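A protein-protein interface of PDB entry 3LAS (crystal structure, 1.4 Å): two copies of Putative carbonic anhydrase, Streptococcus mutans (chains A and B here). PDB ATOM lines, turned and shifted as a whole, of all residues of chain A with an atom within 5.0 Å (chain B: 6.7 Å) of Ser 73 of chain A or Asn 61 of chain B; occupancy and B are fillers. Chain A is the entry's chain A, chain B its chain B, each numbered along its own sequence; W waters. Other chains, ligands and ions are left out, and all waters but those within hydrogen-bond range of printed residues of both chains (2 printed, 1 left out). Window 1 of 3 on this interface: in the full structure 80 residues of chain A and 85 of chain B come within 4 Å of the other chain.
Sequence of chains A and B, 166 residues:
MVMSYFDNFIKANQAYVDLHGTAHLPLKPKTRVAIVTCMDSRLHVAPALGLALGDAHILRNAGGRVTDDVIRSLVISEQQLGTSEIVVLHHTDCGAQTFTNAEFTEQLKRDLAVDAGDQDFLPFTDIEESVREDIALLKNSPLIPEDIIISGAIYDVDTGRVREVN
The side-chain amide nitrogen of Asn 61 of chain B lies within hydrogen-bond range of the side-chain carboxylate of Asp 69 of chain A. The side-chain carboxylate (OD2) of Asp 69 of chain A lies within hydrogen-bond range of the side-chain hydroxyl (OG1) of Thr 67 of chain B (2.7 Å). The side-chain amide nitrogen (ND2) of Asn 61 of chain B sits close to the guanidinium group (NH2) of Arg 72 of chain A (3.4 Å). The guanidinium group (NH2) of Arg 72 of chain A sits at hydrogen-bond distance from the backbone carbonyl oxygen (O) of Ala 62 of chain B (2.9 Å). The guanidinium group (NH1) of Arg 72 of chain A is in hydrogen-bond range of the backbone carbonyl oxygen (O) of Phe 121 of chain B (2.9 Å). OG of Ser 73 of chain A lies within hydrogen-bond range of N of Ala 62 of chain B (2.9 Å). O of Ser 73 of chain A lies close to SD of Met 39 of chain B (3.8 Å).
The guanidinium group (NH2) of Arg 72 of chain A lies within hydrogen-bond range of the side-chain hydroxyl (OG) of Ser 73 of chain A, 3.5 Å away. The backbone carbonyl oxygen (O) of Asn 61 of chain B sits close to the side-chain sulfur (SG) of Cys 38 of chain B (3.7 Å). The backbone NH of Met 39 of chain B sits at hydrogen-bond distance from the backbone carbonyl oxygen of Asn 61 of chain B, 2.8 Å away. The backbone carbonyl oxygen (O) of Asp 40 of chain B is in hydrogen-bond range of the guanidinium group (NH2) of Arg 60 of chain B. The side-chain amide nitrogen (ND2) of Asn 61 of chain B lies within hydrogen-bond range of the backbone carbonyl oxygen (O) of Arg 65 of chain B (2.9 Å). NH1 of Arg 65 of chain B sits at hydrogen-bond distance from O of Leu 122 of chain B (3.1 Å).
Met 39 of chain B touches Leu 59 of chain A (SD to CD1, 3.9 Å). Leu 59 of chain A touches Arg 60 of chain B. CB of Asp 69 of chain A touches CB of Asp 69 of chain B (3.7 Å). Val 70 of chain B touches Asp 69 of chain A (CG2 to OD2, 3.99 Å). Asp 69 of chain B touches Val 70 of chain A. Arg 72 of chain A touches Gln 119 of chain B (CB to OE1, 3.99 Å). Leu 122 of chain B touches Arg 72 of chain A (CB to NH1, 3.8 Å). Asn 61 of chain B touches Ser 73 of chain A. Ile 76 of chain A touches Ala 62 of chain B. Ile 76 of chain A touches Phe 121 of chain B.
Printed residues of chain B within 4 Å of Ser 73 of chain A: Met 39 (3.5 Å), Asn 61 (3.5 Å) and Ala 62 (2.9 Å). Of chain A, only Asp 69, Arg 72 and Ser 73 come within 4 Å of Asn 61 of chain B. Printed residues of chain B within 4 Å of Val 70 of chain A: Asp 69 (3.9 Å). Of the printed residues of chain A, Gln 119 of chain B touches Arg 72. Of the printed residues of chain B, Ile 76 of chain A touches Ala 62 (3.7 Å) and Phe 121 (3.8 Å). The nearest printed residue of chain A that does not touch Gln 119 of chain B is Asp 68 of chain A (4.8 Å).
Printed residues of chain A that touch a printed residue of chain B: Leu 59, Asp 69, Val 70, Arg 72, Ser 73, Ile 76 and Ser 77. Of the 19 printed residues of chain B, 10 touch a printed residue of chain A. Among the printed residues, 18 pairs touch across the chains. Among the printed residues, no Asp or Glu carboxylate lies within 4 Å of a Lys or Arg side-chain nitrogen of the other chain.
Asp 69 of chain A touches its own counterpart, Asp 69 of chain B. Asp 69 of chain A touches Val 70 of chain B, and with the chains exchanged Val 70 of chain A touches Asp 69 of chain B. Positions printed for both chains: 59, 69 and 70.
Water W2 lies within hydrogen-bond range of OD2 of Asp 69 of chain B (2.7 Å) and OD2 of Asp 69 of chain A (2.7 Å). Water W1 lies within hydrogen-bond range of the backbone carbonyl oxygen of Asp 68 of chain A (2.9 Å) and the side-chain amide oxygen of Gln 119 of chain B (2.9 Å).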
ATOM      1  N   LEU A  59     -36.179  -2.760  -2.362  1.00  0.00           N
ATOM      2  CA  LEU A  59     -34.765  -2.974  -1.999  1.00  0.00           C
ATOM      3  C   LEU A  59     -34.617  -4.409  -1.597  1.00  0.00           C
ATOM      4  O   LEU A  59     -35.432  -4.925  -0.815  1.00  0.00           O
ATOM      5  CB  LEU A  59     -34.291  -2.074  -0.864  1.00  0.00           C
ATOM      6  CG  LEU A  59     -34.220  -0.574  -1.166  1.00  0.00           C
ATOM      7  CD1 LEU A  59     -35.597   0.082  -1.298  1.00  0.00           C
ATOM      8  CD2 LEU A  59     -33.549   0.114   0.001  1.00  0.00           C
ATOM      9  N   ASP A  68     -25.403  -0.432   5.520  1.00  0.00           N
ATOM     10  CA  ASP A  68     -25.094   0.905   5.020  1.00  0.00           C
ATOM     11  C   ASP A  68     -25.659   1.133   3.631  1.00  0.00           C
ATOM     12  O   ASP A  68     -26.113   2.249   3.353  1.00  0.00           O
ATOM     13  CB  ASP A  68     -23.576   1.187   5.007  1.00  0.00           C
ATOM     14  CG  ASP A  68     -22.980   1.336   6.413  1.00  0.00           C
ATOM     15  OD1 ASP A  68     -23.667   1.506   7.392  1.00  0.00           O
ATOM     16  OD2 ASP A  68     -21.716   1.323   6.455  1.00  0.00           O
ATOM     17  N   ASP A  69     -25.668   0.142   2.752  1.00  0.00           N
ATOM     18  CA  ASP A  69     -26.231   0.316   1.423  1.00  0.00           C
ATOM     19  C   ASP A  69     -27.734   0.467   1.477  1.00  0.00           C
ATOM     20  O   ASP A  69     -28.293   1.279   0.742  1.00  0.00           O
ATOM     21  CB  ASP A  69     -25.847  -0.922   0.569  1.00  0.00           C
ATOM     22  CG  ASP A  69     -26.163  -0.772  -0.896  1.00  0.00           C
ATOM     23  OD1 ASP A  69     -26.412   0.350  -1.401  1.00  0.00           O
ATOM     24  OD2 ASP A  69     -26.149  -1.806  -1.594  1.00  0.00           O
ATOM     25  N   VAL A  70     -28.432  -0.262   2.352  1.00  0.00           N
ATOM     26  CA  VAL A  70     -29.881  -0.095   2.490  1.00  0.00           C
ATOM     27  C   VAL A  70     -30.126   1.304   2.983  1.00  0.00           C
ATOM     28  O   VAL A  70     -31.037   1.955   2.429  1.00  0.00           O
ATOM     29  CB  VAL A  70     -30.452  -1.170   3.403  1.00  0.00           C
ATOM     30  CG1 VAL A  70     -31.887  -0.793   3.796  1.00  0.00           C
ATOM     31  CG2 VAL A  70     -30.383  -2.549   2.693  1.00  0.00           C
ATOM     32  N   ILE A  71     -29.396   1.818   3.937  1.00  0.00           N
ATOM     33  CA  ILE A  71     -29.635   3.200   4.441  1.00  0.00           C
ATOM     34  C   ILE A  71     -29.310   4.183   3.317  1.00  0.00           C
ATOM     35  O   ILE A  71     -30.106   5.115   3.070  1.00  0.00           O
ATOM     36  CB  ILE A  71     -28.840   3.443   5.677  1.00  0.00           C
ATOM     37  CG1 ILE A  71     -29.491   2.605   6.799  1.00  0.00           C
ATOM     38  CG2 ILE A  71     -28.855   4.965   5.993  1.00  0.00           C
ATOM     39  CD1 ILE A  71     -28.802   2.449   8.115  1.00  0.00           C
ATOM     40  N   ARG A  72     -28.199   4.017   2.561  1.00  0.00           N
ATOM     41  CA  ARG A  72     -27.935   4.892   1.448  1.00  0.00           C
ATOM     42  C   ARG A  72     -29.113   4.959   0.487  1.00  0.00           C
ATOM     43  O   ARG A  72     -29.522   6.034   0.003  1.00  0.00           O
ATOM     44  CB  ARG A  72     -26.667   4.375   0.727  1.00  0.00           C
ATOM     45  CG  ARG A  72     -26.313   5.119  -0.580  1.00  0.00           C
ATOM     46  CD  ARG A  72     -25.293   4.360  -1.381  1.00  0.00           C
ATOM     47  NE  ARG A  72     -25.844   3.162  -2.024  1.00  0.00           N
ATOM     48  CZ  ARG A  72     -26.359   3.113  -3.254  1.00  0.00           C
ATOM     49  NH1 ARG A  72     -26.508   4.160  -4.052  1.00  0.00           N
ATOM     50  NH2 ARG A  72     -26.768   1.939  -3.732  1.00  0.00           N
ATOM     51  N   SER A  73     -29.617   3.767   0.179  1.00  0.00           N
ATOM     52  CA  SER A  73     -30.676   3.655  -0.787  1.00  0.00           C
ATOM     53  C   SER A  73     -31.976   4.261  -0.280  1.00  0.00           C
ATOM     54  O   SER A  73     -32.731   4.873  -1.078  1.00  0.00           O
ATOM     55  CB  SER A  73     -30.855   2.193  -1.193  1.00  0.00           C
ATOM     56  OG  SER A  73     -29.649   1.677  -1.784  1.00  0.00           O
ATOM     57  N   LEU A  74     -32.273   4.068   0.999  1.00  0.00           N
ATOM     58  CA  LEU A  74     -33.442   4.658   1.572  1.00  0.00           C
ATOM     59  C   LEU A  74     -33.343   6.154   1.645  1.00  0.00           C
ATOM     60  O   LEU A  74     -34.377   6.834   1.489  1.00  0.00           O
ATOM     61  CB  LEU A  74     -33.749   4.075   2.975  1.00  0.00           C
ATOM     62  CG  LEU A  74     -34.181   2.637   2.997  1.00  0.00           C
ATOM     63  CD1 LEU A  74     -34.229   2.103   4.411  1.00  0.00           C
ATOM     64  CD2 LEU A  74     -35.581   2.506   2.333  1.00  0.00           C
ATOM     65  N   VAL A  75     -32.173   6.738   1.940  1.00  0.00           N
ATOM     66  CA  VAL A  75     -32.067   8.208   1.997  1.00  0.00           C
ATOM     67  C   VAL A  75     -32.295   8.712   0.577  1.00  0.00           C
ATOM     68  O   VAL A  75     -33.007   9.775   0.390  1.00  0.00           O
ATOM     69  CB  VAL A  75     -30.657   8.576   2.497  1.00  0.00           C
ATOM     70  CG1 VAL A  75     -30.391  10.110   2.195  1.00  0.00           C
ATOM     71  CG2 VAL A  75     -30.466   8.206   3.920  1.00  0.00           C
ATOM     72  N   ILE A  76     -31.844   8.063  -0.488  1.00  0.00           N
ATOM     73  CA  ILE A  76     -32.176   8.493  -1.853  1.00  0.00           C
ATOM     74  C   ILE A  76     -33.655   8.322  -2.060  1.00  0.00           C
ATOM     75  O   ILE A  76     -34.355   9.256  -2.579  1.00  0.00           O
ATOM     76  CB  ILE A  76     -31.312   7.679  -2.886  1.00  0.00           C
ATOM     77  CG1 ILE A  76     -29.870   8.103  -2.725  1.00  0.00           C
ATOM     78  CG2 ILE A  76     -31.858   7.904  -4.293  1.00  0.00           C
ATOM     79  CD1 ILE A  76     -28.908   7.079  -3.415  1.00  0.00           C
ATOM     80  N   SER A  77     -34.229   7.194  -1.697  1.00  0.00           N
ATOM     81  CA  SER A  77     -35.680   6.980  -1.903  1.00  0.00           C
ATOM     82  C   SER A  77     -36.545   8.059  -1.246  1.00  0.00           C
ATOM     83  O   SER A  77     -37.530   8.484  -1.842  1.00  0.00           O
ATOM     84  CB  SER A  77     -36.011   5.580  -1.295  1.00  0.00           C
ATOM     85  OG  SER A  77     -37.393   5.296  -1.403  1.00  0.00           O
ATOM     86  N   VAL B  36     -28.625  -8.090 -10.264  1.00  0.00           N
ATOM     87  CA  VAL B  36     -28.329  -6.873  -9.469  1.00  0.00           C
ATOM     88  C   VAL B  36     -28.913  -5.727 -10.178  1.00  0.00           C
ATOM     89  O   VAL B  36     -28.522  -5.401 -11.337  1.00  0.00           O
ATOM     90  CB  VAL B  36     -26.815  -6.693  -9.291  1.00  0.00           C
ATOM     91  CG1 VAL B  36     -26.507  -5.423  -8.509  1.00  0.00           C
ATOM     92  CG2 VAL B  36     -26.136  -7.890  -8.572  1.00  0.00           C
ATOM     93  N   THR B  37     -29.866  -5.035  -9.574  1.00  0.00           N
ATOM     94  CA  THR B  37     -30.508  -3.920 -10.283  1.00  0.00           C
ATOM     95  C   THR B  37     -30.966  -2.828  -9.338  1.00  0.00           C
ATOM     96  O   THR B  37     -30.668  -2.873  -8.113  1.00  0.00           O
ATOM     97  CB  THR B  37     -31.652  -4.481 -11.174  1.00  0.00           C
ATOM     98  OG1 THR B  37     -32.147  -3.509 -12.083  1.00  0.00           O
ATOM     99  CG2 THR B  37     -32.809  -4.993 -10.329  1.00  0.00           C
ATOM    100  N   CYS B  38     -31.663  -1.826  -9.865  1.00  0.00           N
ATOM    101  CA  CYS B  38     -32.146  -0.717  -9.062  1.00  0.00           C
ATOM    102  C   CYS B  38     -33.440  -0.984  -8.442  1.00  0.00           C
ATOM    103  O   CYS B  38     -34.270  -1.806  -8.930  1.00  0.00           O
ATOM    104  CB  CYS B  38     -32.267   0.505  -9.964  1.00  0.00           C
ATOM    105  SG  CYS B  38     -32.707   2.062  -9.068  1.00  0.00           S
ATOM    106  N   MET B  39     -33.693  -0.354  -7.274  1.00  0.00           N
ATOM    107  CA  MET B  39     -34.960  -0.345  -6.558  1.00  0.00           C
ATOM    108  C   MET B  39     -36.171   0.244  -7.287  1.00  0.00           C
ATOM    109  O   MET B  39     -37.282   0.177  -6.763  1.00  0.00           O
ATOM    110  CB  MET B  39     -34.744   0.348  -5.231  1.00  0.00           C
ATOM    111  CG  MET B  39     -34.544   1.859  -5.394  1.00  0.00           C
ATOM    112  SD  MET B  39     -34.034   2.622  -3.841  1.00  0.00           S
ATOM    113  CE  MET B  39     -33.945   4.308  -4.347  1.00  0.00           C
ATOM    114  N   ASP B  40     -35.932   0.920  -8.408  1.00  0.00           N
ATOM    115  CA  ASP B  40     -36.937   1.697  -9.121  1.00  0.00           C
ATOM    116  C   ASP B  40     -38.294   1.020  -9.157  1.00  0.00           C
ATOM    117  O   ASP B  40     -38.436  -0.141  -9.593  1.00  0.00           O
ATOM    118  CB  ASP B  40     -36.441   1.990 -10.546  1.00  0.00           C
ATOM    119  CG  ASP B  40     -37.256   3.065 -11.216  1.00  0.00           C
ATOM    120  OD1 ASP B  40     -38.329   2.696 -11.764  1.00  0.00           O
ATOM    121  OD2 ASP B  40     -36.777   4.227 -11.230  1.00  0.00           O
ATOM    122  N   LEU B  59     -31.392  -8.826  -6.447  1.00  0.00           N
ATOM    123  CA  LEU B  59     -30.766  -7.881  -5.497  1.00  0.00           C
ATOM    124  C   LEU B  59     -31.097  -6.496  -6.030  1.00  0.00           C
ATOM    125  O   LEU B  59     -30.959  -6.243  -7.237  1.00  0.00           O
ATOM    126  CB  LEU B  59     -29.262  -8.052  -5.420  1.00  0.00           C
ATOM    127  CG  LEU B  59     -28.761  -9.351  -4.779  1.00  0.00           C
ATOM    128  CD1 LEU B  59     -28.962 -10.619  -5.623  1.00  0.00           C
ATOM    129  CD2 LEU B  59     -27.218  -9.179  -4.554  1.00  0.00           C
ATOM    130  N   ARG B  60     -31.510  -5.588  -5.159  1.00  0.00           N
ATOM    131  CA  ARG B  60     -31.914  -4.245  -5.637  1.00  0.00           C
ATOM    132  C   ARG B  60     -31.458  -3.223  -4.637  1.00  0.00           C
ATOM    133  O   ARG B  60     -31.692  -3.350  -3.397  1.00  0.00           O
ATOM    134  CB  ARG B  60     -33.433  -4.123  -5.817  1.00  0.00           C
ATOM    135  CG  ARG B  60     -34.013  -5.253  -6.710  1.00  0.00           C
ATOM    136  CD  ARG B  60     -35.523  -5.119  -7.016  1.00  0.00           C
ATOM    137  NE  ARG B  60     -35.742  -3.971  -7.911  1.00  0.00           N
ATOM    138  CZ  ARG B  60     -36.886  -3.739  -8.529  1.00  0.00           C
ATOM    139  NH1 ARG B  60     -37.898  -4.543  -8.459  1.00  0.00           N
ATOM    140  NH2 ARG B  60     -36.961  -2.673  -9.278  1.00  0.00           N
ATOM    141  N   ASN B  61     -30.879  -2.117  -5.128  1.00  0.00           N
ATOM    142  CA  ASN B  61     -30.489  -0.998  -4.259  1.00  0.00           C
ATOM    143  C   ASN B  61     -30.670   0.252  -5.098  1.00  0.00           C
ATOM    144  O   ASN B  61     -31.141   0.196  -6.231  1.00  0.00           O
ATOM    145  CB  ASN B  61     -29.060  -1.193  -3.693  1.00  0.00           C
ATOM    146  CG  ASN B  61     -27.996  -1.125  -4.750  1.00  0.00           C
ATOM    147  OD1 ASN B  61     -28.258  -0.792  -5.922  1.00  0.00           O
ATOM    148  ND2 ASN B  61     -26.798  -1.440  -4.349  1.00  0.00           N
ATOM    149  N   ALA B  62     -30.261   1.415  -4.572  1.00  0.00           N
ATOM    150  CA  ALA B  62     -30.348   2.634  -5.416  1.00  0.00           C
ATOM    151  C   ALA B  62     -29.295   2.627  -6.495  1.00  0.00           C
ATOM    152  O   ALA B  62     -28.095   2.618  -6.217  1.00  0.00           O
ATOM    153  CB  ALA B  62     -30.180   3.838  -4.524  1.00  0.00           C
ATOM    154  N   GLY B  63     -29.758   2.574  -7.738  1.00  0.00           N
ATOM    155  CA  GLY B  63     -28.869   2.557  -8.908  1.00  0.00           C
ATOM    156  C   GLY B  63     -28.457   1.206  -9.411  1.00  0.00           C
ATOM    157  O   GLY B  63     -27.886   1.114 -10.510  1.00  0.00           O
ATOM    158  N   GLY B  64     -28.631   0.133  -8.638  1.00  0.00           N
ATOM    159  CA  GLY B  64     -28.076  -1.154  -9.016  1.00  0.00           C
ATOM    160  C   GLY B  64     -26.563  -1.166  -8.923  1.00  0.00           C
ATOM    161  O   GLY B  64     -25.882  -1.813  -9.735  1.00  0.00           O
ATOM    162  N   ARG B  65     -26.017  -0.465  -7.926  1.00  0.00           N
ATOM    163  CA  ARG B  65     -24.554  -0.298  -7.819  1.00  0.00           C
ATOM    164  C   ARG B  65     -23.928  -1.430  -7.030  1.00  0.00           C
ATOM    165  O   ARG B  65     -24.519  -1.942  -6.036  1.00  0.00           O
ATOM    166  CB  ARG B  65     -24.269   1.027  -7.133  1.00  0.00           C
ATOM    167  CG  ARG B  65     -24.883   2.247  -7.739  1.00  0.00           C
ATOM    168  CD  ARG B  65     -24.797   2.410  -9.237  1.00  0.00           C
ATOM    169  NE  ARG B  65     -23.512   2.084  -9.887  1.00  0.00           N
ATOM    170  CZ  ARG B  65     -22.576   2.994 -10.159  1.00  0.00           C
ATOM    171  NH1 ARG B  65     -22.642   4.216  -9.662  1.00  0.00           N
ATOM    172  NH2 ARG B  65     -21.557   2.567 -10.819  1.00  0.00           N
ATOM    173  N   VAL B  66     -22.713  -1.808  -7.350  1.00  0.00           N
ATOM    174  CA  VAL B  66     -21.994  -2.788  -6.535  1.00  0.00           C
ATOM    175  C   VAL B  66     -21.437  -2.122  -5.318  1.00  0.00           C
ATOM    176  O   VAL B  66     -20.748  -1.061  -5.425  1.00  0.00           O
ATOM    177  CB  VAL B  66     -20.950  -3.492  -7.403  1.00  0.00           C
ATOM    178  CG1 VAL B  66     -20.088  -4.434  -6.546  1.00  0.00           C
ATOM    179  CG2 VAL B  66     -21.642  -4.341  -8.444  1.00  0.00           C
ATOM    180  N   THR B  67     -21.791  -2.640  -4.163  1.00  0.00           N
ATOM    181  CA  THR B  67     -21.418  -2.142  -2.835  1.00  0.00           C
ATOM    182  C   THR B  67     -20.931  -3.330  -2.019  1.00  0.00           C
ATOM    183  O   THR B  67     -21.092  -4.508  -2.402  1.00  0.00           O
ATOM    184  CB  THR B  67     -22.631  -1.539  -2.131  1.00  0.00           C
ATOM    185  OG1 THR B  67     -23.587  -2.651  -1.949  1.00  0.00           O
ATOM    186  CG2 THR B  67     -23.302  -0.384  -2.939  1.00  0.00           C
ATOM    187  N   ASP B  69     -22.535  -4.550   0.514  1.00  0.00           N
ATOM    188  CA  ASP B  69     -23.727  -5.369   0.731  1.00  0.00           C
ATOM    189  C   ASP B  69     -24.070  -6.194  -0.504  1.00  0.00           C
ATOM    190  O   ASP B  69     -24.451  -7.364  -0.336  1.00  0.00           O
ATOM    191  CB  ASP B  69     -24.906  -4.473   1.085  1.00  0.00           C
ATOM    192  CG  ASP B  69     -26.121  -5.200   1.570  1.00  0.00           C
ATOM    193  OD1 ASP B  69     -26.069  -6.379   1.971  1.00  0.00           O
ATOM    194  OD2 ASP B  69     -27.168  -4.512   1.622  1.00  0.00           O
ATOM    195  N   VAL B  70     -23.913  -5.669  -1.696  1.00  0.00           N
ATOM    196  CA  VAL B  70     -24.126  -6.503  -2.871  1.00  0.00           C
ATOM    197  C   VAL B  70     -23.144  -7.623  -2.919  1.00  0.00           C
ATOM    198  O   VAL B  70     -23.546  -8.765  -3.221  1.00  0.00           O
ATOM    199  CB  VAL B  70     -24.094  -5.614  -4.134  1.00  0.00           C
ATOM    200  CG1 VAL B  70     -24.077  -6.502  -5.419  1.00  0.00           C
ATOM    201  CG2 VAL B  70     -25.332  -4.721  -4.192  1.00  0.00           C
ATOM    202  N   GLN B 119     -19.972  10.744   2.642  1.00  0.00           N
ATOM    203  CA  GLN B 119     -20.584   9.501   2.218  1.00  0.00           C
ATOM    204  C   GLN B 119     -20.735   9.526   0.723  1.00  0.00           C
ATOM    205  O   GLN B 119     -21.010  10.548   0.137  1.00  0.00           O
ATOM    206  CB  GLN B 119     -21.963   9.338   2.858  1.00  0.00           C
ATOM    207  CG  GLN B 119     -22.860   8.276   2.249  1.00  0.00           C
ATOM    208  CD  GLN B 119     -23.865   7.804   3.276  1.00  0.00           C
ATOM    209  OE1 GLN B 119     -24.565   6.817   3.084  1.00  0.00           O
ATOM    210  NE2 GLN B 119     -23.916   8.517   4.394  1.00  0.00           N
ATOM    211  N   PHE B 121     -22.811   8.423  -2.305  1.00  0.00           N
ATOM    212  CA  PHE B 121     -24.167   7.982  -2.686  1.00  0.00           C
ATOM    213  C   PHE B 121     -24.147   7.262  -4.014  1.00  0.00           C
ATOM    214  O   PHE B 121     -25.220   6.765  -4.425  1.00  0.00           O
ATOM    215  CB  PHE B 121     -25.132   9.208  -2.671  1.00  0.00           C
ATOM    216  CG  PHE B 121     -25.384   9.630  -1.274  1.00  0.00           C
ATOM    217  CD1 PHE B 121     -26.353   9.012  -0.479  1.00  0.00           C
ATOM    218  CD2 PHE B 121     -24.639  10.687  -0.748  1.00  0.00           C
ATOM    219  CE1 PHE B 121     -26.573   9.405   0.860  1.00  0.00           C
ATOM    220  CE2 PHE B 121     -24.891  11.086   0.615  1.00  0.00           C
ATOM    221  CZ  PHE B 121     -25.826  10.422   1.352  1.00  0.00           C
ATOM    222  N   LEU B 122     -22.990   7.160  -4.687  1.00  0.00           N
ATOM    223  CA  LEU B 122     -22.825   6.307  -5.900  1.00  0.00           C
ATOM    224  C   LEU B 122     -23.654   6.774  -7.079  1.00  0.00           C
ATOM    225  O   LEU B 122     -24.301   5.925  -7.741  1.00  0.00           O
ATOM    226  CB  LEU B 122     -23.041   4.802  -5.592  1.00  0.00           C
ATOM    227  CG  LEU B 122     -22.151   4.266  -4.463  1.00  0.00           C
ATOM    228  CD1 LEU B 122     -22.552   2.779  -4.143  1.00  0.00           C
ATOM    229  CD2 LEU B 122     -20.684   4.327  -4.758  1.00  0.00           C
HETATM  230  O   HOH W   1     -25.471   4.655   4.788  1.00  0.00           O
HETATM  231  O   HOH W   2     -28.027  -3.649  -0.826  1.00  0.00           O
